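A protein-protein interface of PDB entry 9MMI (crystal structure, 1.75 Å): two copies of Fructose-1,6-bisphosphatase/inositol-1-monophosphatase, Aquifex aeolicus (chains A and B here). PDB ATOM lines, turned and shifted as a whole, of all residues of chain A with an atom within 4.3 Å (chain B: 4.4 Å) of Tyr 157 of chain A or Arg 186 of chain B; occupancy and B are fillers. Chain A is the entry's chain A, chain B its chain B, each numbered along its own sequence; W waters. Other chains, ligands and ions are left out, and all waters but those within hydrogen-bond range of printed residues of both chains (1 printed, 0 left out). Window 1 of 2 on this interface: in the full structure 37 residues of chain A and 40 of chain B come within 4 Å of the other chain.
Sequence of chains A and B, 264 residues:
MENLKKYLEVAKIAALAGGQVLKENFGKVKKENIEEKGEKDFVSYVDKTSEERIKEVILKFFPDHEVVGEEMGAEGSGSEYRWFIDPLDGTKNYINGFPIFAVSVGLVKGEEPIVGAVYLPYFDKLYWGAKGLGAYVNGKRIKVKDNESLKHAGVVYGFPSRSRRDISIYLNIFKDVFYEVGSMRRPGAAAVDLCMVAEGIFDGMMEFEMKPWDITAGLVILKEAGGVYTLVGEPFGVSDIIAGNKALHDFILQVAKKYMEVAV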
ATOM      1  N   VAL A 155      -4.564  18.644  10.402  1.00  0.00           N
ATOM      2  CA  VAL A 155      -5.322  17.763  11.283  1.00  0.00           C
ATOM      3  C   VAL A 155      -5.266  16.335  10.757  1.00  0.00           C
ATOM      4  O   VAL A 155      -5.486  16.081   9.555  1.00  0.00           O
ATOM      5  CB  VAL A 155      -6.786  18.259  11.429  1.00  0.00           C
ATOM      6  CG1 VAL A 155      -7.576  17.287  12.240  1.00  0.00           C
ATOM      7  CG2 VAL A 155      -6.864  19.658  12.042  1.00  0.00           C
ATOM      8  N   VAL A 156      -4.920  15.383  11.650  1.00  0.00           N
ATOM      9  CA  VAL A 156      -4.986  13.971  11.303  1.00  0.00           C
ATOM     10  C   VAL A 156      -6.307  13.405  11.809  1.00  0.00           C
ATOM     11  O   VAL A 156      -6.829  13.802  12.860  1.00  0.00           O
ATOM     12  CB  VAL A 156      -3.792  13.141  11.812  1.00  0.00           C
ATOM     13  CG1 VAL A 156      -2.655  13.310  10.832  1.00  0.00           C
ATOM     14  CG2 VAL A 156      -3.402  13.630  13.172  1.00  0.00           C
ATOM     15  N   TYR A 157      -6.872  12.489  11.048  1.00  0.00           N
ATOM     16  CA  TYR A 157      -8.178  11.948  11.398  1.00  0.00           C
ATOM     17  C   TYR A 157      -8.249  10.474  11.064  1.00  0.00           C
ATOM     18  O   TYR A 157      -7.483   9.948  10.242  1.00  0.00           O
ATOM     19  CB  TYR A 157      -9.315  12.717  10.694  1.00  0.00           C
ATOM     20  CG  TYR A 157      -9.403  12.571   9.189  1.00  0.00           C
ATOM     21  CD1 TYR A 157      -8.560  13.275   8.341  1.00  0.00           C
ATOM     22  CD2 TYR A 157     -10.331  11.729   8.612  1.00  0.00           C
ATOM     23  CE1 TYR A 157      -8.655  13.149   6.978  1.00  0.00           C
ATOM     24  CE2 TYR A 157     -10.441  11.589   7.222  1.00  0.00           C
ATOM     25  CZ  TYR A 157      -9.590  12.302   6.412  1.00  0.00           C
ATOM     26  OH  TYR A 157      -9.644  12.210   5.048  1.00  0.00           O
ATOM     27  N   GLY A 158      -9.179   9.820  11.730  1.00  0.00           N
ATOM     28  CA  GLY A 158      -9.563   8.469  11.367  1.00  0.00           C
ATOM     29  C   GLY A 158     -10.923   8.093  11.915  1.00  0.00           C
ATOM     30  O   GLY A 158     -11.360   8.578  12.964  1.00  0.00           O
ATOM     31  N   PHE A 159     -11.591   7.218  11.201  1.00  0.00           N
ATOM     32  CA  PHE A 159     -12.814   6.614  11.721  1.00  0.00           C
ATOM     33  C   PHE A 159     -13.054   5.339  10.935  1.00  0.00           C
ATOM     34  O   PHE A 159     -12.533   5.202   9.807  1.00  0.00           O
ATOM     35  CB  PHE A 159     -14.016   7.571  11.651  1.00  0.00           C
ATOM     36  CG  PHE A 159     -14.241   8.243  10.322  1.00  0.00           C
ATOM     37  CD1 PHE A 159     -14.979   7.647   9.330  1.00  0.00           C
ATOM     38  CD2 PHE A 159     -13.728   9.512  10.089  1.00  0.00           C
ATOM     39  CE1 PHE A 159     -15.183   8.275   8.107  1.00  0.00           C
ATOM     40  CE2 PHE A 159     -13.945  10.178   8.865  1.00  0.00           C
ATOM     41  CZ  PHE A 159     -14.671   9.530   7.867  1.00  0.00           C
ATOM     42  N   PHE A 174     -16.003  15.815   9.718  1.00  0.00           N
ATOM     43  CA  PHE A 174     -14.923  15.976   8.762  1.00  0.00           C
ATOM     44  C   PHE A 174     -15.113  17.209   7.886  1.00  0.00           C
ATOM     45  O   PHE A 174     -14.199  18.019   7.715  1.00  0.00           O
ATOM     46  CB  PHE A 174     -14.790  14.728   7.871  1.00  0.00           C
ATOM     47  CG  PHE A 174     -13.906  14.981   6.681  1.00  0.00           C
ATOM     48  CD1 PHE A 174     -12.545  14.870   6.763  1.00  0.00           C
ATOM     49  CD2 PHE A 174     -14.478  15.397   5.492  1.00  0.00           C
ATOM     50  CE1 PHE A 174     -11.741  15.162   5.670  1.00  0.00           C
ATOM     51  CE2 PHE A 174     -13.717  15.681   4.410  1.00  0.00           C
ATOM     52  CZ  PHE A 174     -12.360  15.589   4.475  1.00  0.00           C
ATOM     53  N   PHE A 178     -12.609  20.308   7.712  1.00  0.00           N
ATOM     54  CA  PHE A 178     -11.948  20.385   6.406  1.00  0.00           C
ATOM     55  C   PHE A 178     -12.096  21.746   5.755  1.00  0.00           C
ATOM     56  O   PHE A 178     -11.144  22.257   5.146  1.00  0.00           O
ATOM     57  CB  PHE A 178     -12.564  19.290   5.546  1.00  0.00           C
ATOM     58  CG  PHE A 178     -11.940  19.068   4.187  1.00  0.00           C
ATOM     59  CD1 PHE A 178     -10.620  18.781   4.044  1.00  0.00           C
ATOM     60  CD2 PHE A 178     -12.767  19.030   3.046  1.00  0.00           C
ATOM     61  CE1 PHE A 178     -10.101  18.481   2.790  1.00  0.00           C
ATOM     62  CE2 PHE A 178     -12.230  18.734   1.804  1.00  0.00           C
ATOM     63  CZ  PHE A 178     -10.904  18.445   1.699  1.00  0.00           C
ATOM     64  N   MET A 184      -6.047  18.107   5.983  1.00  0.00           N
ATOM     65  CA  MET A 184      -6.481  16.933   6.740  1.00  0.00           C
ATOM     66  C   MET A 184      -5.844  15.708   6.133  1.00  0.00           C
ATOM     67  O   MET A 184      -5.816  15.535   4.894  1.00  0.00           O
ATOM     68  CB  MET A 184      -8.021  16.769   6.760  1.00  0.00           C
ATOM     69  CG  MET A 184      -8.663  18.014   7.200  1.00  0.00           C
ATOM     70  SD  MET A 184     -10.251  17.869   7.971  1.00  0.00           S
ATOM     71  CE  MET A 184     -10.202  16.490   9.183  1.00  0.00           C
ATOM     72  N   ARG A 185      -5.335  14.824   7.006  1.00  0.00           N
ATOM     73  CA  ARG A 185      -4.623  13.652   6.549  1.00  0.00           C
ATOM     74  C   ARG A 185      -5.095  12.430   7.313  1.00  0.00           C
ATOM     75  O   ARG A 185      -5.426  12.500   8.501  1.00  0.00           O
ATOM     76  CB  ARG A 185      -3.105  13.852   6.719  1.00  0.00           C
ATOM     77  CG  ARG A 185      -2.522  15.069   5.974  1.00  0.00           C
ATOM     78  CD  ARG A 185      -2.491  14.824   4.469  1.00  0.00           C
ATOM     79  NE  ARG A 185      -2.030  16.022   3.785  1.00  0.00           N
ATOM     80  CZ  ARG A 185      -2.777  16.850   3.082  1.00  0.00           C
ATOM     81  NH1 ARG A 185      -4.091  16.685   2.951  1.00  0.00           N
ATOM     82  NH2 ARG A 185      -2.197  17.879   2.493  1.00  0.00           N
ATOM     83  N   ARG A 186      -5.127  11.291   6.614  1.00  0.00           N
ATOM     84  CA  ARG A 186      -5.640  10.037   7.166  1.00  0.00           C
ATOM     85  C   ARG A 186      -4.558   8.988   6.936  1.00  0.00           C
ATOM     86  O   ARG A 186      -4.558   8.286   5.917  1.00  0.00           O
ATOM     87  CB  ARG A 186      -6.978   9.638   6.536  1.00  0.00           C
ATOM     88  CG  ARG A 186      -7.511   8.297   6.928  1.00  0.00           C
ATOM     89  CD  ARG A 186      -8.774   8.018   6.105  1.00  0.00           C
ATOM     90  NE  ARG A 186      -9.669   7.298   6.961  1.00  0.00           N
ATOM     91  CZ  ARG A 186     -10.934   7.573   7.180  1.00  0.00           C
ATOM     92  NH1 ARG A 186     -11.599   8.498   6.475  1.00  0.00           N
ATOM     93  NH2 ARG A 186     -11.561   6.913   8.131  1.00  0.00           N
ATOM     94  N   ASP A 193      -0.653   8.907  14.767  1.00  0.00           N
ATOM     95  CA  ASP A 193      -1.299  10.228  14.774  1.00  0.00           C
ATOM     96  C   ASP A 193      -1.070  10.988  16.075  1.00  0.00           C
ATOM     97  O   ASP A 193      -0.667  12.153  16.046  1.00  0.00           O
ATOM     98  CB  ASP A 193      -2.787  10.079  14.439  1.00  0.00           C
ATOM     99  CG  ASP A 193      -3.050   9.560  13.027  1.00  0.00           C
ATOM    100  OD1 ASP A 193      -2.134   9.600  12.188  1.00  0.00           O
ATOM    101  OD2 ASP A 193      -4.134   9.129  12.737  1.00  0.00           O
ATOM    102  N   MET A 206      -8.501  13.914  15.344  1.00  0.00           N
ATOM    103  CA  MET A 206      -9.807  13.403  15.731  1.00  0.00           C
ATOM    104  C   MET A 206      -9.886  11.956  15.287  1.00  0.00           C
ATOM    105  O   MET A 206      -9.774  11.668  14.095  1.00  0.00           O
ATOM    106  CB  MET A 206     -10.972  14.180  15.140  1.00  0.00           C
ATOM    107  CG  MET A 206     -10.903  14.345  13.653  1.00  0.00           C
ATOM    108  SD  MET A 206     -12.258  15.408  13.098  1.00  0.00           S
ATOM    109  CE  MET A 206     -12.843  14.454  11.711  1.00  0.00           C
ATOM    110  N   GLU A 207     -10.059  11.041  16.224  1.00  0.00           N
ATOM    111  CA  GLU A 207     -10.096   9.610  15.895  1.00  0.00           C
ATOM    112  C   GLU A 207     -11.271   9.028  16.654  1.00  0.00           C
ATOM    113  O   GLU A 207     -11.417   9.267  17.850  1.00  0.00           O
ATOM    114  CB  GLU A 207      -8.814   8.910  16.256  1.00  0.00           C
ATOM    115  CG  GLU A 207      -7.583   9.651  15.844  1.00  0.00           C
ATOM    116  CD  GLU A 207      -6.838   9.093  14.647  1.00  0.00           C
ATOM    117  OE1 GLU A 207      -7.141   7.985  14.203  1.00  0.00           O
ATOM    118  OE2 GLU A 207      -5.943   9.848  14.148  1.00  0.00           O
ATOM    119  N   TYR B 157      -6.845   8.372  -1.605  1.00  0.00           N
ATOM    120  CA  TYR B 157      -7.774   9.365  -2.124  1.00  0.00           C
ATOM    121  C   TYR B 157      -7.305  10.767  -1.774  1.00  0.00           C
ATOM    122  O   TYR B 157      -6.510  10.986  -0.838  1.00  0.00           O
ATOM    123  CB  TYR B 157      -9.210   9.131  -1.596  1.00  0.00           C
ATOM    124  CG  TYR B 157      -9.423   9.345  -0.113  1.00  0.00           C
ATOM    125  CD1 TYR B 157      -9.052   8.384   0.813  1.00  0.00           C
ATOM    126  CD2 TYR B 157     -10.006  10.498   0.368  1.00  0.00           C
ATOM    127  CE1 TYR B 157      -9.249   8.558   2.143  1.00  0.00           C
ATOM    128  CE2 TYR B 157     -10.213  10.695   1.714  1.00  0.00           C
ATOM    129  CZ  TYR B 157      -9.830   9.719   2.603  1.00  0.00           C
ATOM    130  OH  TYR B 157     -10.009   9.877   3.958  1.00  0.00           O
ATOM    131  N   GLY B 158      -7.829  11.719  -2.521  1.00  0.00           N
ATOM    132  CA  GLY B 158      -7.696  13.119  -2.165  1.00  0.00           C
ATOM    133  C   GLY B 158      -8.728  13.971  -2.868  1.00  0.00           C
ATOM    134  O   GLY B 158      -9.158  13.673  -3.984  1.00  0.00           O
ATOM    135  N   PHE B 159      -9.089  15.062  -2.238  1.00  0.00           N
ATOM    136  CA  PHE B 159      -9.865  16.105  -2.896  1.00  0.00           C
ATOM    137  C   PHE B 159      -9.672  17.385  -2.106  1.00  0.00           C
ATOM    138  O   PHE B 159      -9.316  17.333  -0.917  1.00  0.00           O
ATOM    139  CB  PHE B 159     -11.359  15.733  -3.007  1.00  0.00           C
ATOM    140  CG  PHE B 159     -11.994  15.211  -1.741  1.00  0.00           C
ATOM    141  CD1 PHE B 159     -12.592  16.056  -0.829  1.00  0.00           C
ATOM    142  CD2 PHE B 159     -12.055  13.837  -1.508  1.00  0.00           C
ATOM    143  CE1 PHE B 159     -13.209  15.571   0.314  1.00  0.00           C
ATOM    144  CE2 PHE B 159     -12.648  13.325  -0.354  1.00  0.00           C
ATOM    145  CZ  PHE B 159     -13.232  14.206   0.564  1.00  0.00           C
ATOM    146  N   ARG B 185      -6.891   5.717   2.532  1.00  0.00           N
ATOM    147  CA  ARG B 185      -5.839   6.538   3.106  1.00  0.00           C
ATOM    148  C   ARG B 185      -5.705   7.831   2.328  1.00  0.00           C
ATOM    149  O   ARG B 185      -5.850   7.863   1.101  1.00  0.00           O
ATOM    150  CB  ARG B 185      -4.481   5.765   3.110  1.00  0.00           C
ATOM    151  CG  ARG B 185      -4.501   4.453   3.922  1.00  0.00           C
ATOM    152  CD  ARG B 185      -4.623   4.717   5.420  1.00  0.00           C
ATOM    153  NE  ARG B 185      -4.776   3.450   6.128  1.00  0.00           N
ATOM    154  CZ  ARG B 185      -5.876   2.995   6.699  1.00  0.00           C
ATOM    155  NH1 ARG B 185      -7.031   3.652   6.643  1.00  0.00           N
ATOM    156  NH2 ARG B 185      -5.827   1.827   7.320  1.00  0.00           N
ATOM    157  N   ARG B 186      -5.374   8.911   3.049  1.00  0.00           N
ATOM    158  CA  ARG B 186      -5.246  10.253   2.485  1.00  0.00           C
ATOM    159  C   ARG B 186      -3.889  10.810   2.891  1.00  0.00           C
ATOM    160  O   ARG B 186      -3.758  11.475   3.932  1.00  0.00           O
ATOM    161  CB  ARG B 186      -6.390  11.145   2.930  1.00  0.00           C
ATOM    162  CG  ARG B 186      -6.404  12.503   2.360  1.00  0.00           C
ATOM    163  CD  ARG B 186      -7.457  13.232   3.186  1.00  0.00           C
ATOM    164  NE  ARG B 186      -7.849  14.363   2.413  1.00  0.00           N
ATOM    165  CZ  ARG B 186      -9.062  14.594   1.966  1.00  0.00           C
ATOM    166  NH1 ARG B 186     -10.138  14.045   2.534  1.00  0.00           N
ATOM    167  NH2 ARG B 186      -9.203  15.394   0.931  1.00  0.00           N
ATOM    168  N   PRO B 187      -2.841  10.545   2.092  1.00  0.00           N
ATOM    169  CA  PRO B 187      -1.496  10.963   2.510  1.00  0.00           C
ATOM    170  C   PRO B 187      -1.150  12.380   2.089  1.00  0.00           C
ATOM    171  O   PRO B 187      -0.188  12.918   2.653  1.00  0.00           O
ATOM    172  CB  PRO B 187      -0.593   9.932   1.815  1.00  0.00           C
ATOM    173  CG  PRO B 187      -1.571   8.716   1.506  1.00  0.00           C
ATOM    174  CD  PRO B 187      -2.758   9.495   1.047  1.00  0.00           C
ATOM    175  N   GLY B 188      -1.867  12.963   1.112  1.00  0.00           N
ATOM    176  CA  GLY B 188      -1.663  14.356   0.791  1.00  0.00           C
ATOM    177  C   GLY B 188      -0.693  14.717  -0.317  1.00  0.00           C
ATOM    178  O   GLY B 188      -0.282  15.881  -0.391  1.00  0.00           O
HETATM  179  O   HOH W   1       0.385  18.159   1.260  1.00  0.00           O
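Tyr 157 of chain A touches two residues of chain B. Of chain A, only Tyr 157, Phe 174, Phe 178, Met 184, Arg 185 and Arg 186 come within 4 Å of Arg 186 of chain B. Printed residues of chain B within 4 Å of Arg 186 of chain A: Tyr 157, Arg 185 and Arg 186. Of the printed residues of chain A, Pro 187 of chain B touches Arg 185. Of the printed residues of chain A, Arg 185 of chain B touches Arg 186 (3.5 Å). Of the printed residues of chain B, Met 184 of chain A touches Arg 186. Of the printed residues of chain B, Arg 185 of chain A touches Arg 186, Pro 187 and Gly 188. Val 155 of chain A touches none of the printed residues of chain B. Met 206 of chain A touches none of the printed residues of chain B.
The side-chain hydroxyl (OH) of Tyr 157 of chain A lies within hydrogen-bond range of the side-chain hydroxyl (OH) of Tyr 157 of chain B (2.6 Å). The side-chain hydroxyl (OH) of Tyr 157 of chain A sits close to the guanidinium group (NH1) of Arg 186 of chain B, at 3.2 Å. O of Met 184 of chain A lies close to NE of Arg 186 of chain B, 3.4 Å away. OH of Tyr 157 of chain B sits close to NH1 of Arg 186 of chain A (3.3 Å). The backbone carbonyl oxygen of Arg 186 of chain B sits at hydrogen-bond distance from the backbone NH of Arg 186 of chain A (3.0 Å).
Of the 13 printed residues of chain A, 6 touch a printed residue of chain B. Printed residues of chain B that touch a printed residue of chain A: Tyr 157, Phe 159, Arg 185, Arg 186, Pro 187 and Gly 188. Among the printed residues, 12 pairs touch across the chains. Among the printed residues, no Asp or Glu carboxylate lies within 4 Å of a Lys or Arg side-chain nitrogen of the other chain.
NH1 of Arg 186 of chain B touches CZ of Phe 174 of chain A (3.3 Å). Phe 159 of chain B touches Phe 178 of chain A (O to CZ, 3.3 Å). CZ of Phe 178 of chain A touches NH2 of Arg 186 of chain B, at 3.6 Å. Arg 185 of chain A touches Arg 186 of chain B (CA to O, 3.5 Å). Pro 187 of chain B touches Arg 185 of chain A (O to CD, 3.5 Å). NE of Arg 185 of chain A touches CA of Gly 188 of chain B, 3.4 Å away. Arg 186 of chain A touches Arg 185 of chain B.
Water W1 bridges the guanidinium group of Arg 185 of chain A (2.9 Å) and the backbone carbonyl oxygen of Gly 188 of chain B (2.9 Å).
Tyr 157 of chain A touches its own counterpart, Tyr 157 of chain B. Tyr 157 of chain A touches Arg 186 of chain B, and with the chains exchanged Arg 186 of chain A touches Tyr 157 of chain B. Arg 185 of chain A touches Arg 186 of chain B, and with the chains exchanged Arg 186 of chain A touches Arg 185 of chain B. Arg 186 of chain B touches its own counterpart, Arg 186 of chain A.
The backbone carbonyl oxygen (O) of Val 155 of chain A sits at hydrogen-bond distance from the backbone NH (N) of Arg 185 of chain A, 2.8 Å away. O of Arg 185 of chain A sits at hydrogen-bond distance from N of Tyr 157 of chain A. The guanidinium group (NH2) of Arg 186 of chain A lies within hydrogen-bond range of the backbone carbonyl oxygen (O) of Phe 159 of chain A (2.6 Å). The side-chain sulfur (SD) of Met 184 of chain A lies within hydrogen-bond range of the backbone NH (N) of Phe 178 of chain A (3.4 Å). The backbone carbonyl oxygen (O) of Arg 185 of chain B sits at hydrogen-bond distance from the backbone NH (N) of Tyr 157 of chain B (2.9 Å). The backbone carbonyl oxygen (O) of Phe 159 of chain B lies within hydrogen-bond range of the guanidinium group (NH2) of Arg 186 of chain B (2.7 Å).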
